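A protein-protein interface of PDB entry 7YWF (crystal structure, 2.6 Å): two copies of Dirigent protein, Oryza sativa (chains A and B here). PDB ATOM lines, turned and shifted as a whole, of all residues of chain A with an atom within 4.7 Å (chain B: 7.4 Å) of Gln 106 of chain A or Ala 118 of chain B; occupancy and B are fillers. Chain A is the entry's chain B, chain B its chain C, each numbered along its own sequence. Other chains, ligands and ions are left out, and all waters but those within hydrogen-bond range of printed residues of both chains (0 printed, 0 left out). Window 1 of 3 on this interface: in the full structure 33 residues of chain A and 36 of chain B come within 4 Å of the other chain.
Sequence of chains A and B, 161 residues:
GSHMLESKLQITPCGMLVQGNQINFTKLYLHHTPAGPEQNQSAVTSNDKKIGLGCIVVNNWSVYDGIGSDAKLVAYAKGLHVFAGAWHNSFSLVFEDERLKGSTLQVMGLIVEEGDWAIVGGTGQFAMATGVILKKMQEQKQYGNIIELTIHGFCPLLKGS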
ATOM      1  N   PHE A  91      12.143 -15.316 -13.684  1.00  0.00           N
ATOM      2  CA  PHE A  91      12.672 -14.964 -14.991  1.00  0.00           C
ATOM      3  C   PHE A  91      13.424 -16.144 -15.589  1.00  0.00           C
ATOM      4  O   PHE A  91      13.806 -17.088 -14.892  1.00  0.00           O
ATOM      5  CB  PHE A  91      13.572 -13.722 -14.902  1.00  0.00           C
ATOM      6  CG  PHE A  91      14.781 -13.899 -14.026  1.00  0.00           C
ATOM      7  CD1 PHE A  91      15.960 -14.421 -14.534  1.00  0.00           C
ATOM      8  CD2 PHE A  91      14.740 -13.530 -12.690  1.00  0.00           C
ATOM      9  CE1 PHE A  91      17.071 -14.577 -13.727  1.00  0.00           C
ATOM     10  CE2 PHE A  91      15.848 -13.684 -11.878  1.00  0.00           C
ATOM     11  CZ  PHE A  91      17.015 -14.206 -12.397  1.00  0.00           C
ATOM     12  N   SER A  92      13.632 -16.068 -16.899  1.00  0.00           N
ATOM     13  CA  SER A  92      14.412 -17.044 -17.645  1.00  0.00           C
ATOM     14  C   SER A  92      15.787 -16.460 -17.944  1.00  0.00           C
ATOM     15  O   SER A  92      15.894 -15.432 -18.621  1.00  0.00           O
ATOM     16  CB  SER A  92      13.709 -17.430 -18.947  1.00  0.00           C
ATOM     17  OG  SER A  92      12.438 -18.002 -18.700  1.00  0.00           O
ATOM     18  N   THR A 104      18.752 -22.286 -21.375  1.00  0.00           N
ATOM     19  CA  THR A 104      18.277 -21.298 -20.420  1.00  0.00           C
ATOM     20  C   THR A 104      18.287 -21.883 -19.013  1.00  0.00           C
ATOM     21  O   THR A 104      18.334 -23.101 -18.820  1.00  0.00           O
ATOM     22  CB  THR A 104      16.861 -20.815 -20.760  1.00  0.00           C
ATOM     23  OG1 THR A 104      15.928 -21.887 -20.571  1.00  0.00           O
ATOM     24  CG2 THR A 104      16.789 -20.344 -22.204  1.00  0.00           C
ATOM     25  N   LEU A 105      18.243 -20.990 -18.027  1.00  0.00           N
ATOM     26  CA  LEU A 105      18.124 -21.361 -16.623  1.00  0.00           C
ATOM     27  C   LEU A 105      16.936 -20.613 -16.043  1.00  0.00           C
ATOM     28  O   LEU A 105      16.897 -19.379 -16.087  1.00  0.00           O
ATOM     29  CB  LEU A 105      19.398 -21.032 -15.840  1.00  0.00           C
ATOM     30  CG  LEU A 105      20.604 -21.952 -16.019  1.00  0.00           C
ATOM     31  CD1 LEU A 105      21.827 -21.352 -15.349  1.00  0.00           C
ATOM     32  CD2 LEU A 105      20.299 -23.319 -15.431  1.00  0.00           C
ATOM     33  N   GLN A 106      15.973 -21.353 -15.506  1.00  0.00           N
ATOM     34  CA  GLN A 106      14.791 -20.751 -14.910  1.00  0.00           C
ATOM     35  C   GLN A 106      15.068 -20.443 -13.445  1.00  0.00           C
ATOM     36  O   GLN A 106      15.492 -21.322 -12.687  1.00  0.00           O
ATOM     37  CB  GLN A 106      13.588 -21.683 -15.052  1.00  0.00           C
ATOM     38  CG  GLN A 106      13.307 -22.083 -16.492  1.00  0.00           C
ATOM     39  CD  GLN A 106      13.120 -20.891 -17.410  1.00  0.00           C
ATOM     40  OE1 GLN A 106      12.498 -19.897 -17.041  1.00  0.00           O
ATOM     41  NE2 GLN A 106      13.673 -20.983 -18.614  1.00  0.00           N
ATOM     42  N   VAL A 107      14.830 -19.195 -13.051  1.00  0.00           N
ATOM     43  CA  VAL A 107      15.233 -18.693 -11.744  1.00  0.00           C
ATOM     44  C   VAL A 107      14.014 -18.097 -11.056  1.00  0.00           C
ATOM     45  O   VAL A 107      13.251 -17.347 -11.674  1.00  0.00           O
ATOM     46  CB  VAL A 107      16.359 -17.648 -11.854  1.00  0.00           C
ATOM     47  CG1 VAL A 107      16.789 -17.184 -10.472  1.00  0.00           C
ATOM     48  CG2 VAL A 107      17.541 -18.214 -12.627  1.00  0.00           C
ATOM     49  N   MET A 108      13.827 -18.446  -9.786  1.00  0.00           N
ATOM     50  CA  MET A 108      12.813 -17.842  -8.938  1.00  0.00           C
ATOM     51  C   MET A 108      13.420 -17.587  -7.566  1.00  0.00           C
ATOM     52  O   MET A 108      14.355 -18.277  -7.154  1.00  0.00           O
ATOM     53  CB  MET A 108      11.568 -18.735  -8.842  1.00  0.00           C
ATOM     54  CG  MET A 108      10.387 -18.091  -8.143  1.00  0.00           C
ATOM     55  SD  MET A 108       8.941 -19.158  -8.080  1.00  0.00           S
ATOM     56  CE  MET A 108       8.338 -18.951  -9.749  1.00  0.00           C
ATOM     57  N   ALA A 118      16.727 -19.116  -6.406  1.00  0.00           N
ATOM     58  CA  ALA A 118      16.613 -20.556  -6.591  1.00  0.00           C
ATOM     59  C   ALA A 118      16.591 -20.886  -8.076  1.00  0.00           C
ATOM     60  O   ALA A 118      15.832 -20.283  -8.843  1.00  0.00           O
ATOM     61  CB  ALA A 118      15.356 -21.099  -5.910  1.00  0.00           C
ATOM     62  N   ILE A 119      17.430 -21.837  -8.477  1.00  0.00           N
ATOM     63  CA  ILE A 119      17.389 -22.381  -9.829  1.00  0.00           C
ATOM     64  C   ILE A 119      16.335 -23.483  -9.837  1.00  0.00           C
ATOM     65  O   ILE A 119      16.560 -24.577  -9.314  1.00  0.00           O
ATOM     66  CB  ILE A 119      18.758 -22.908 -10.269  1.00  0.00           C
ATOM     67  CG1 ILE A 119      19.793 -21.781 -10.224  1.00  0.00           C
ATOM     68  CG2 ILE A 119      18.676 -23.507 -11.664  1.00  0.00           C
ATOM     69  CD1 ILE A 119      21.197 -22.224 -10.556  1.00  0.00           C
ATOM     70  N   VAL A 120      15.178 -23.195 -10.438  1.00  0.00           N
ATOM     71  CA  VAL A 120      14.037 -24.097 -10.382  1.00  0.00           C
ATOM     72  C   VAL A 120      13.931 -24.984 -11.612  1.00  0.00           C
ATOM     73  O   VAL A 120      13.060 -25.862 -11.657  1.00  0.00           O
ATOM     74  CB  VAL A 120      12.731 -23.301 -10.187  1.00  0.00           C
ATOM     75  CG1 VAL A 120      12.811 -22.464  -8.921  1.00  0.00           C
ATOM     76  CG2 VAL A 120      12.468 -22.415 -11.391  1.00  0.00           C
ATOM     77  N   GLY A 121      14.806 -24.806 -12.592  1.00  0.00           N
ATOM     78  CA  GLY A 121      14.741 -25.603 -13.798  1.00  0.00           C
ATOM     79  C   GLY A 121      15.622 -25.007 -14.875  1.00  0.00           C
ATOM     80  O   GLY A 121      16.367 -24.054 -14.639  1.00  0.00           O
ATOM     81  N   GLY A 122      15.521 -25.591 -16.061  1.00  0.00           N
ATOM     82  CA  GLY A 122      16.276 -25.098 -17.197  1.00  0.00           C
ATOM     83  C   GLY A 122      15.896 -25.857 -18.447  1.00  0.00           C
ATOM     84  O   GLY A 122      15.122 -26.819 -18.410  1.00  0.00           O
ATOM     85  N   THR A 123      16.467 -25.413 -19.565  1.00  0.00           N
ATOM     86  CA  THR A 123      16.208 -26.008 -20.866  1.00  0.00           C
ATOM     87  C   THR A 123      17.524 -26.204 -21.605  1.00  0.00           C
ATOM     88  O   THR A 123      18.559 -25.644 -21.237  1.00  0.00           O
ATOM     89  CB  THR A 123      15.268 -25.131 -21.703  1.00  0.00           C
ATOM     90  OG1 THR A 123      15.827 -23.819 -21.838  1.00  0.00           O
ATOM     91  CG2 THR A 123      13.906 -25.018 -21.039  1.00  0.00           C
ATOM     92  N   HIS B  88       8.352 -14.643 -21.463  1.00  0.00           N
ATOM     93  CA  HIS B  88       8.668 -15.524 -20.347  1.00  0.00           C
ATOM     94  C   HIS B  88       7.385 -16.133 -19.801  1.00  0.00           C
ATOM     95  O   HIS B  88       6.433 -15.411 -19.490  1.00  0.00           O
ATOM     96  CB  HIS B  88       9.399 -14.752 -19.248  1.00  0.00           C
ATOM     97  CG  HIS B  88       9.596 -15.532 -17.987  1.00  0.00           C
ATOM     98  ND1 HIS B  88      10.445 -16.614 -17.903  1.00  0.00           N
ATOM     99  CD2 HIS B  88       9.043 -15.391 -16.758  1.00  0.00           C
ATOM    100  CE1 HIS B  88      10.414 -17.100 -16.674  1.00  0.00           C
ATOM    101  NE2 HIS B  88       9.570 -16.378 -15.961  1.00  0.00           N
ATOM    102  N   ASN B  89       7.359 -17.458 -19.692  1.00  0.00           N
ATOM    103  CA  ASN B  89       6.153 -18.179 -19.319  1.00  0.00           C
ATOM    104  C   ASN B  89       6.265 -18.746 -17.910  1.00  0.00           C
ATOM    105  O   ASN B  89       7.350 -19.108 -17.446  1.00  0.00           O
ATOM    106  CB  ASN B  89       5.869 -19.314 -20.305  1.00  0.00           C
ATOM    107  CG  ASN B  89       5.375 -18.810 -21.643  1.00  0.00           C
ATOM    108  OD1 ASN B  89       4.172 -18.687 -21.866  1.00  0.00           O
ATOM    109  ND2 ASN B  89       6.306 -18.515 -22.543  1.00  0.00           N
ATOM    110  N   PHE B  91       3.248 -21.138 -15.672  1.00  0.00           N
ATOM    111  CA  PHE B  91       1.861 -21.578 -15.611  1.00  0.00           C
ATOM    112  C   PHE B  91       1.800 -22.990 -15.049  1.00  0.00           C
ATOM    113  O   PHE B  91       2.804 -23.704 -14.992  1.00  0.00           O
ATOM    114  CB  PHE B  91       1.193 -21.522 -16.992  1.00  0.00           C
ATOM    115  CG  PHE B  91       1.716 -22.544 -17.965  1.00  0.00           C
ATOM    116  CD1 PHE B  91       2.804 -22.260 -18.770  1.00  0.00           C
ATOM    117  CD2 PHE B  91       1.105 -23.783 -18.088  1.00  0.00           C
ATOM    118  CE1 PHE B  91       3.285 -23.197 -19.668  1.00  0.00           C
ATOM    119  CE2 PHE B  91       1.580 -24.723 -18.981  1.00  0.00           C
ATOM    120  CZ  PHE B  91       2.671 -24.429 -19.774  1.00  0.00           C
ATOM    121  N   LEU B 105       1.457 -29.895 -13.739  1.00  0.00           N
ATOM    122  CA  LEU B 105       2.866 -29.780 -14.098  1.00  0.00           C
ATOM    123  C   LEU B 105       3.231 -28.306 -14.129  1.00  0.00           C
ATOM    124  O   LEU B 105       2.682 -27.546 -14.934  1.00  0.00           O
ATOM    125  CB  LEU B 105       3.155 -30.430 -15.455  1.00  0.00           C
ATOM    126  CG  LEU B 105       3.087 -31.953 -15.529  1.00  0.00           C
ATOM    127  CD1 LEU B 105       3.231 -32.422 -16.966  1.00  0.00           C
ATOM    128  CD2 LEU B 105       4.199 -32.529 -14.679  1.00  0.00           C
ATOM    129  N   GLN B 106       4.149 -27.903 -13.259  1.00  0.00           N
ATOM    130  CA  GLN B 106       4.574 -26.512 -13.208  1.00  0.00           C
ATOM    131  C   GLN B 106       5.624 -26.263 -14.282  1.00  0.00           C
ATOM    132  O   GLN B 106       6.639 -26.964 -14.345  1.00  0.00           O
ATOM    133  CB  GLN B 106       5.117 -26.173 -11.824  1.00  0.00           C
ATOM    134  CG  GLN B 106       4.094 -26.373 -10.721  1.00  0.00           C
ATOM    135  CD  GLN B 106       2.793 -25.646 -10.995  1.00  0.00           C
ATOM    136  OE1 GLN B 106       1.713 -26.229 -10.907  1.00  0.00           O
ATOM    137  NE2 GLN B 106       2.888 -24.365 -11.328  1.00  0.00           N
ATOM    138  N   VAL B 107       5.381 -25.262 -15.124  1.00  0.00           N
ATOM    139  CA  VAL B 107       6.173 -25.034 -16.326  1.00  0.00           C
ATOM    140  C   VAL B 107       6.658 -23.592 -16.327  1.00  0.00           C
ATOM    141  O   VAL B 107       5.869 -22.665 -16.108  1.00  0.00           O
ATOM    142  CB  VAL B 107       5.362 -25.332 -17.602  1.00  0.00           C
ATOM    143  CG1 VAL B 107       6.239 -25.204 -18.839  1.00  0.00           C
ATOM    144  CG2 VAL B 107       4.727 -26.713 -17.522  1.00  0.00           C
ATOM    145  N   MET B 108       7.951 -23.407 -16.580  1.00  0.00           N
ATOM    146  CA  MET B 108       8.543 -22.090 -16.755  1.00  0.00           C
ATOM    147  C   MET B 108       9.507 -22.133 -17.930  1.00  0.00           C
ATOM    148  O   MET B 108      10.181 -23.143 -18.149  1.00  0.00           O
ATOM    149  CB  MET B 108       9.282 -21.641 -15.489  1.00  0.00           C
ATOM    150  CG  MET B 108       9.785 -20.214 -15.544  1.00  0.00           C
ATOM    151  SD  MET B 108      10.709 -19.736 -14.076  1.00  0.00           S
ATOM    152  CE  MET B 108       9.557 -20.215 -12.803  1.00  0.00           C
ATOM    153  N   GLY B 109       9.569 -21.044 -18.681  1.00  0.00           N
ATOM    154  CA  GLY B 109      10.489 -20.970 -19.797  1.00  0.00           C
ATOM    155  C   GLY B 109      10.139 -19.820 -20.716  1.00  0.00           C
ATOM    156  O   GLY B 109       9.201 -19.059 -20.476  1.00  0.00           O
ATOM    157  N   LEU B 110      10.929 -19.711 -21.780  1.00  0.00           N
ATOM    158  CA  LEU B 110      10.834 -18.613 -22.728  1.00  0.00           C
ATOM    159  C   LEU B 110      10.220 -19.093 -24.036  1.00  0.00           C
ATOM    160  O   LEU B 110      10.308 -20.274 -24.387  1.00  0.00           O
ATOM    161  CB  LEU B 110      12.212 -18.003 -23.000  1.00  0.00           C
ATOM    162  CG  LEU B 110      12.271 -16.492 -23.243  1.00  0.00           C
ATOM    163  CD1 LEU B 110      11.914 -15.729 -21.981  1.00  0.00           C
ATOM    164  CD2 LEU B 110      13.648 -16.088 -23.744  1.00  0.00           C
ATOM    165  N   ASP B 116      12.087 -24.340 -26.049  1.00  0.00           N
ATOM    166  CA  ASP B 116      11.985 -25.301 -24.965  1.00  0.00           C
ATOM    167  C   ASP B 116      11.338 -24.662 -23.744  1.00  0.00           C
ATOM    168  O   ASP B 116      11.481 -23.462 -23.496  1.00  0.00           O
ATOM    169  CB  ASP B 116      13.362 -25.865 -24.583  1.00  0.00           C
ATOM    170  CG  ASP B 116      13.990 -26.687 -25.693  1.00  0.00           C
ATOM    171  OD1 ASP B 116      13.314 -26.942 -26.709  1.00  0.00           O
ATOM    172  OD2 ASP B 116      15.166 -27.085 -25.543  1.00  0.00           O
ATOM    173  N   TRP B 117      10.620 -25.487 -22.988  1.00  0.00           N
ATOM    174  CA  TRP B 117      10.082 -25.132 -21.686  1.00  0.00           C
ATOM    175  C   TRP B 117      10.703 -26.036 -20.633  1.00  0.00           C
ATOM    176  O   TRP B 117      11.184 -27.130 -20.933  1.00  0.00           O
ATOM    177  CB  TRP B 117       8.555 -25.267 -21.643  1.00  0.00           C
ATOM    178  CG  TRP B 117       7.801 -24.050 -22.070  1.00  0.00           C
ATOM    179  CD1 TRP B 117       8.257 -22.765 -22.092  1.00  0.00           C
ATOM    180  CD2 TRP B 117       6.445 -24.004 -22.528  1.00  0.00           C
ATOM    181  NE1 TRP B 117       7.268 -21.921 -22.538  1.00  0.00           N
ATOM    182  CE2 TRP B 117       6.146 -22.657 -22.814  1.00  0.00           C
ATOM    183  CE3 TRP B 117       5.455 -24.972 -22.728  1.00  0.00           C
ATOM    184  CZ2 TRP B 117       4.898 -22.254 -23.288  1.00  0.00           C
ATOM    185  CZ3 TRP B 117       4.217 -24.570 -23.199  1.00  0.00           C
ATOM    186  CH2 TRP B 117       3.950 -23.223 -23.474  1.00  0.00           C
ATOM    187  N   ALA B 118      10.704 -25.563 -19.392  1.00  0.00           N
ATOM    188  CA  ALA B 118      11.278 -26.298 -18.276  1.00  0.00           C
ATOM    189  C   ALA B 118      10.186 -26.726 -17.308  1.00  0.00           C
ATOM    190  O   ALA B 118       9.284 -25.946 -16.986  1.00  0.00           O
ATOM    191  CB  ALA B 118      12.324 -25.457 -17.538  1.00  0.00           C
ATOM    192  N   ILE B 119      10.270 -27.969 -16.848  1.00  0.00           N
ATOM    193  CA  ILE B 119       9.364 -28.487 -15.832  1.00  0.00           C
ATOM    194  C   ILE B 119      10.010 -28.262 -14.474  1.00  0.00           C
ATOM    195  O   ILE B 119      11.067 -28.828 -14.173  1.00  0.00           O
ATOM    196  CB  ILE B 119       9.058 -29.973 -16.062  1.00  0.00           C
ATOM    197  CG1 ILE B 119       8.346 -30.162 -17.400  1.00  0.00           C
ATOM    198  CG2 ILE B 119       8.225 -30.531 -14.918  1.00  0.00           C
ATOM    199  CD1 ILE B 119       8.074 -31.602 -17.731  1.00  0.00           C
ATOM    200  N   VAL B 120       9.377 -27.427 -13.653  1.00  0.00           N
ATOM    201  CA  VAL B 120       9.941 -27.010 -12.378  1.00  0.00           C
ATOM    202  C   VAL B 120       9.251 -27.662 -11.195  1.00  0.00           C
ATOM    203  O   VAL B 120       9.681 -27.458 -10.051  1.00  0.00           O
ATOM    204  CB  VAL B 120       9.908 -25.478 -12.244  1.00  0.00           C
ATOM    205  CG1 VAL B 120      10.640 -24.840 -13.414  1.00  0.00           C
ATOM    206  CG2 VAL B 120       8.480 -24.995 -12.209  1.00  0.00           C
ATOM    207  N   GLY B 121       8.214 -28.459 -11.429  1.00  0.00           N
ATOM    208  CA  GLY B 121       7.510 -29.106 -10.342  1.00  0.00           C
ATOM    209  C   GLY B 121       6.231 -29.744 -10.845  1.00  0.00           C
ATOM    210  O   GLY B 121       5.952 -29.760 -12.045  1.00  0.00           O
ATOM    211  N   THR B 130      10.401 -33.039 -12.581  1.00  0.00           N
ATOM    212  CA  THR B 130      11.477 -32.228 -13.130  1.00  0.00           C
ATOM    213  C   THR B 130      11.753 -32.693 -14.550  1.00  0.00           C
ATOM    214  O   THR B 130      11.802 -33.896 -14.820  1.00  0.00           O
ATOM    215  CB  THR B 130      12.752 -32.313 -12.275  1.00  0.00           C
ATOM    216  OG1 THR B 130      13.829 -31.649 -12.948  1.00  0.00           O
ATOM    217  CG2 THR B 130      13.136 -33.762 -12.008  1.00  0.00           C
ATOM    218  N   GLY B 131      11.918 -31.736 -15.458  1.00  0.00           N
ATOM    219  CA  GLY B 131      12.162 -32.078 -16.845  1.00  0.00           C
ATOM    220  C   GLY B 131      12.002 -30.866 -17.738  1.00  0.00           C
ATOM    221  O   GLY B 131      12.111 -29.725 -17.287  1.00  0.00           O
ATOM    222  N   VAL B 132      11.749 -31.139 -19.018  1.00  0.00           N
ATOM    223  CA  VAL B 132      11.620 -30.103 -20.031  1.00  0.00           C
ATOM    224  C   VAL B 132      10.415 -30.414 -20.907  1.00  0.00           C
ATOM    225  O   VAL B 132       9.972 -31.560 -21.017  1.00  0.00           O
ATOM    226  CB  VAL B 132      12.888 -29.970 -20.906  1.00  0.00           C
ATOM    227  CG1 VAL B 132      14.079 -29.536 -20.066  1.00  0.00           C
ATOM    228  CG2 VAL B 132      13.181 -31.279 -21.623  1.00  0.00           C
ATOM    229  N   ILE B 133       9.882 -29.368 -21.532  1.00  0.00           N
ATOM    230  CA  ILE B 133       8.789 -29.481 -22.487  1.00  0.00           C
ATOM    231  C   ILE B 133       9.264 -28.907 -23.813  1.00  0.00           C
ATOM    232  O   ILE B 133       9.747 -27.770 -23.866  1.00  0.00           O
ATOM    233  CB  ILE B 133       7.516 -28.762 -22.006  1.00  0.00           C
ATOM    234  CG1 ILE B 133       6.993 -29.406 -20.721  1.00  0.00           C
ATOM    235  CG2 ILE B 133       6.450 -28.775 -23.092  1.00  0.00           C
ATOM    236  CD1 ILE B 133       5.666 -28.852 -20.268  1.00  0.00           C
ATOM    237  N   LEU B 134       9.124 -29.691 -24.876  1.00  0.00           N
ATOM    238  CA  LEU B 134       9.485 -29.261 -26.216  1.00  0.00           C
ATOM    239  C   LEU B 134       8.241 -28.755 -26.931  1.00  0.00           C
ATOM    240  O   LEU B 134       7.152 -29.312 -26.773  1.00  0.00           O
ATOM    241  CB  LEU B 134      10.123 -30.403 -27.008  1.00  0.00           C
ATOM    242  CG  LEU B 134      11.353 -31.056 -26.371  1.00  0.00           C
ATOM    243  CD1 LEU B 134      11.918 -32.138 -27.278  1.00  0.00           C
ATOM    244  CD2 LEU B 134      12.412 -30.015 -26.041  1.00  0.00           C
ATOM    245  N   LYS B 135       8.408 -27.691 -27.710  1.00  0.00           N
ATOM    246  CA  LYS B 135       7.309 -27.074 -28.432  1.00  0.00           C
ATOM    247  C   LYS B 135       7.575 -27.138 -29.929  1.00  0.00           C
ATOM    248  O   LYS B 135       8.727 -27.148 -30.373  1.00  0.00           O
ATOM    249  CB  LYS B 135       7.108 -25.617 -27.997  1.00  0.00           C
ATOM    250  CG  LYS B 135       6.604 -25.460 -26.571  1.00  0.00           C
ATOM    251  CD  LYS B 135       6.891 -24.069 -26.032  1.00  0.00           C
ATOM    252  CE  LYS B 135       8.377 -23.866 -25.793  1.00  0.00           C
ATOM    253  NZ  LYS B 135       8.683 -22.466 -25.386  1.00  0.00           N
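The side-chain amide oxygen (OE1) of Gln 106 of chain A sits close to the side-chain sulfur (SD) of Met 108 of chain B (3.5 Å). The side-chain hydroxyl (OG) of Ser 92 of chain A lies within hydrogen-bond range of a ring nitrogen (ND1) of His 88 of chain B (2.6 Å).
N of Thr 123 of chain A is in hydrogen-bond range of O of Thr 104 of chain A (3.1 Å). The backbone carbonyl oxygen of Gly 109 of chain B lies within hydrogen-bond range of the backbone NH of Asn 89 of chain B, at 2.6 Å. O of Gly 121 of chain A sits at hydrogen-bond distance from N of Gln 106 of chain A, 2.9 Å away. O of Phe 91 of chain A is in hydrogen-bond range of N of Val 107 of chain A, 3.0 Å away. The backbone carbonyl oxygen (O) of Gln 106 of chain A is in hydrogen-bond range of the backbone NH (N) of Val 120 of chain A, at 2.9 Å. N of Ala 118 of chain A lies within hydrogen-bond range of O of Met 108 of chain A (2.6 Å).
Among the printed residues, merely in contact across the chains: Phe 91 of chain A with His 88 of chain B (3.3 Å), Ser 92 of chain A with Gly 109 of chain B (3.6 Å), Ser 92 of chain A with Leu 110 of chain B (3.8 Å), Gln 106 of chain A with His 88 of chain B (3.5 Å), Gln 106 of chain A with Gly 109 of chain B (3.4 Å), Gln 106 of chain A with Ala 118 of chain B (3.7 Å), Met 108 of chain A with Met 108 of chain B (3.5 Å), Val 120 of chain A with Met 108 of chain B (3.9 Å), Val 120 of chain A with Val 120 of chain B (3.2 Å), Gly 122 of chain A with Ala 118 of chain B (3.2 Å), Gly 122 of chain A with Val 132 of chain B (3.3 Å), Thr 123 of chain A with Asp 116 of chain B (3.5 Å), Thr 123 of chain A with Trp 117 of chain B (3.4 Å) and Thr 123 of chain A with Ala 118 of chain B (3.6 Å).
Gln 106 of chain A touches four residues of chain B. Ala 118 of chain B touches three residues of chain A. Of the printed residues of chain B, Thr 123 of chain A touches Asp 116, Trp 117 and Ala 118. Of the printed residues of chain A, Asp 116 of chain B touches Thr 123 (3.5 Å). Printed residues of chain A within 4 Å of Val 132 of chain B: Gly 122. The nearest residue of chain B that does not touch Gln 106 of chain A is Leu 110 of chain B (4.4 Å).
Of the 13 printed residues of chain A, 7 touch a printed residue of chain B. Of the 21 printed residues of chain B, 9 touch a printed residue of chain A. Printed residues of chain B that touch a printed residue of chain A: His 88, Met 108, Gly 109, Leu 110, Asp 116, Trp 117, Ala 118, Val 120 and Val 132. Hydrophobic or aromatic side chains of chain B within 4 Å of the printed part of chain A: His 88, Met 108, Leu 110, Ala 118, Val 120 and Val 132. Among the printed residues, 16 pairs touch across the chains. Among the printed residues, no Asp or Glu carboxylate lies within 4 Å of a Lys or Arg side-chain nitrogen of the other chain.
Gln 106 of chain A touches Ala 118 of chain B, but with the chains exchanged Ala 118 of chain A does not touch Gln 106 of chain B (12.6 Å). Met 108 of chain B touches its own counterpart, Met 108 of chain A. Val 120 of chain A touches Met 108 of chain B, but with the chains exchanged Met 108 of chain A does not touch Val 120 of chain B (6.5 Å). Val 120 of chain B touches its own counterpart, Val 120 of chain A. Of the 16 pairs that touch across the chains among the printed residues, 2 have their exchanged pair printed and touching as well.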
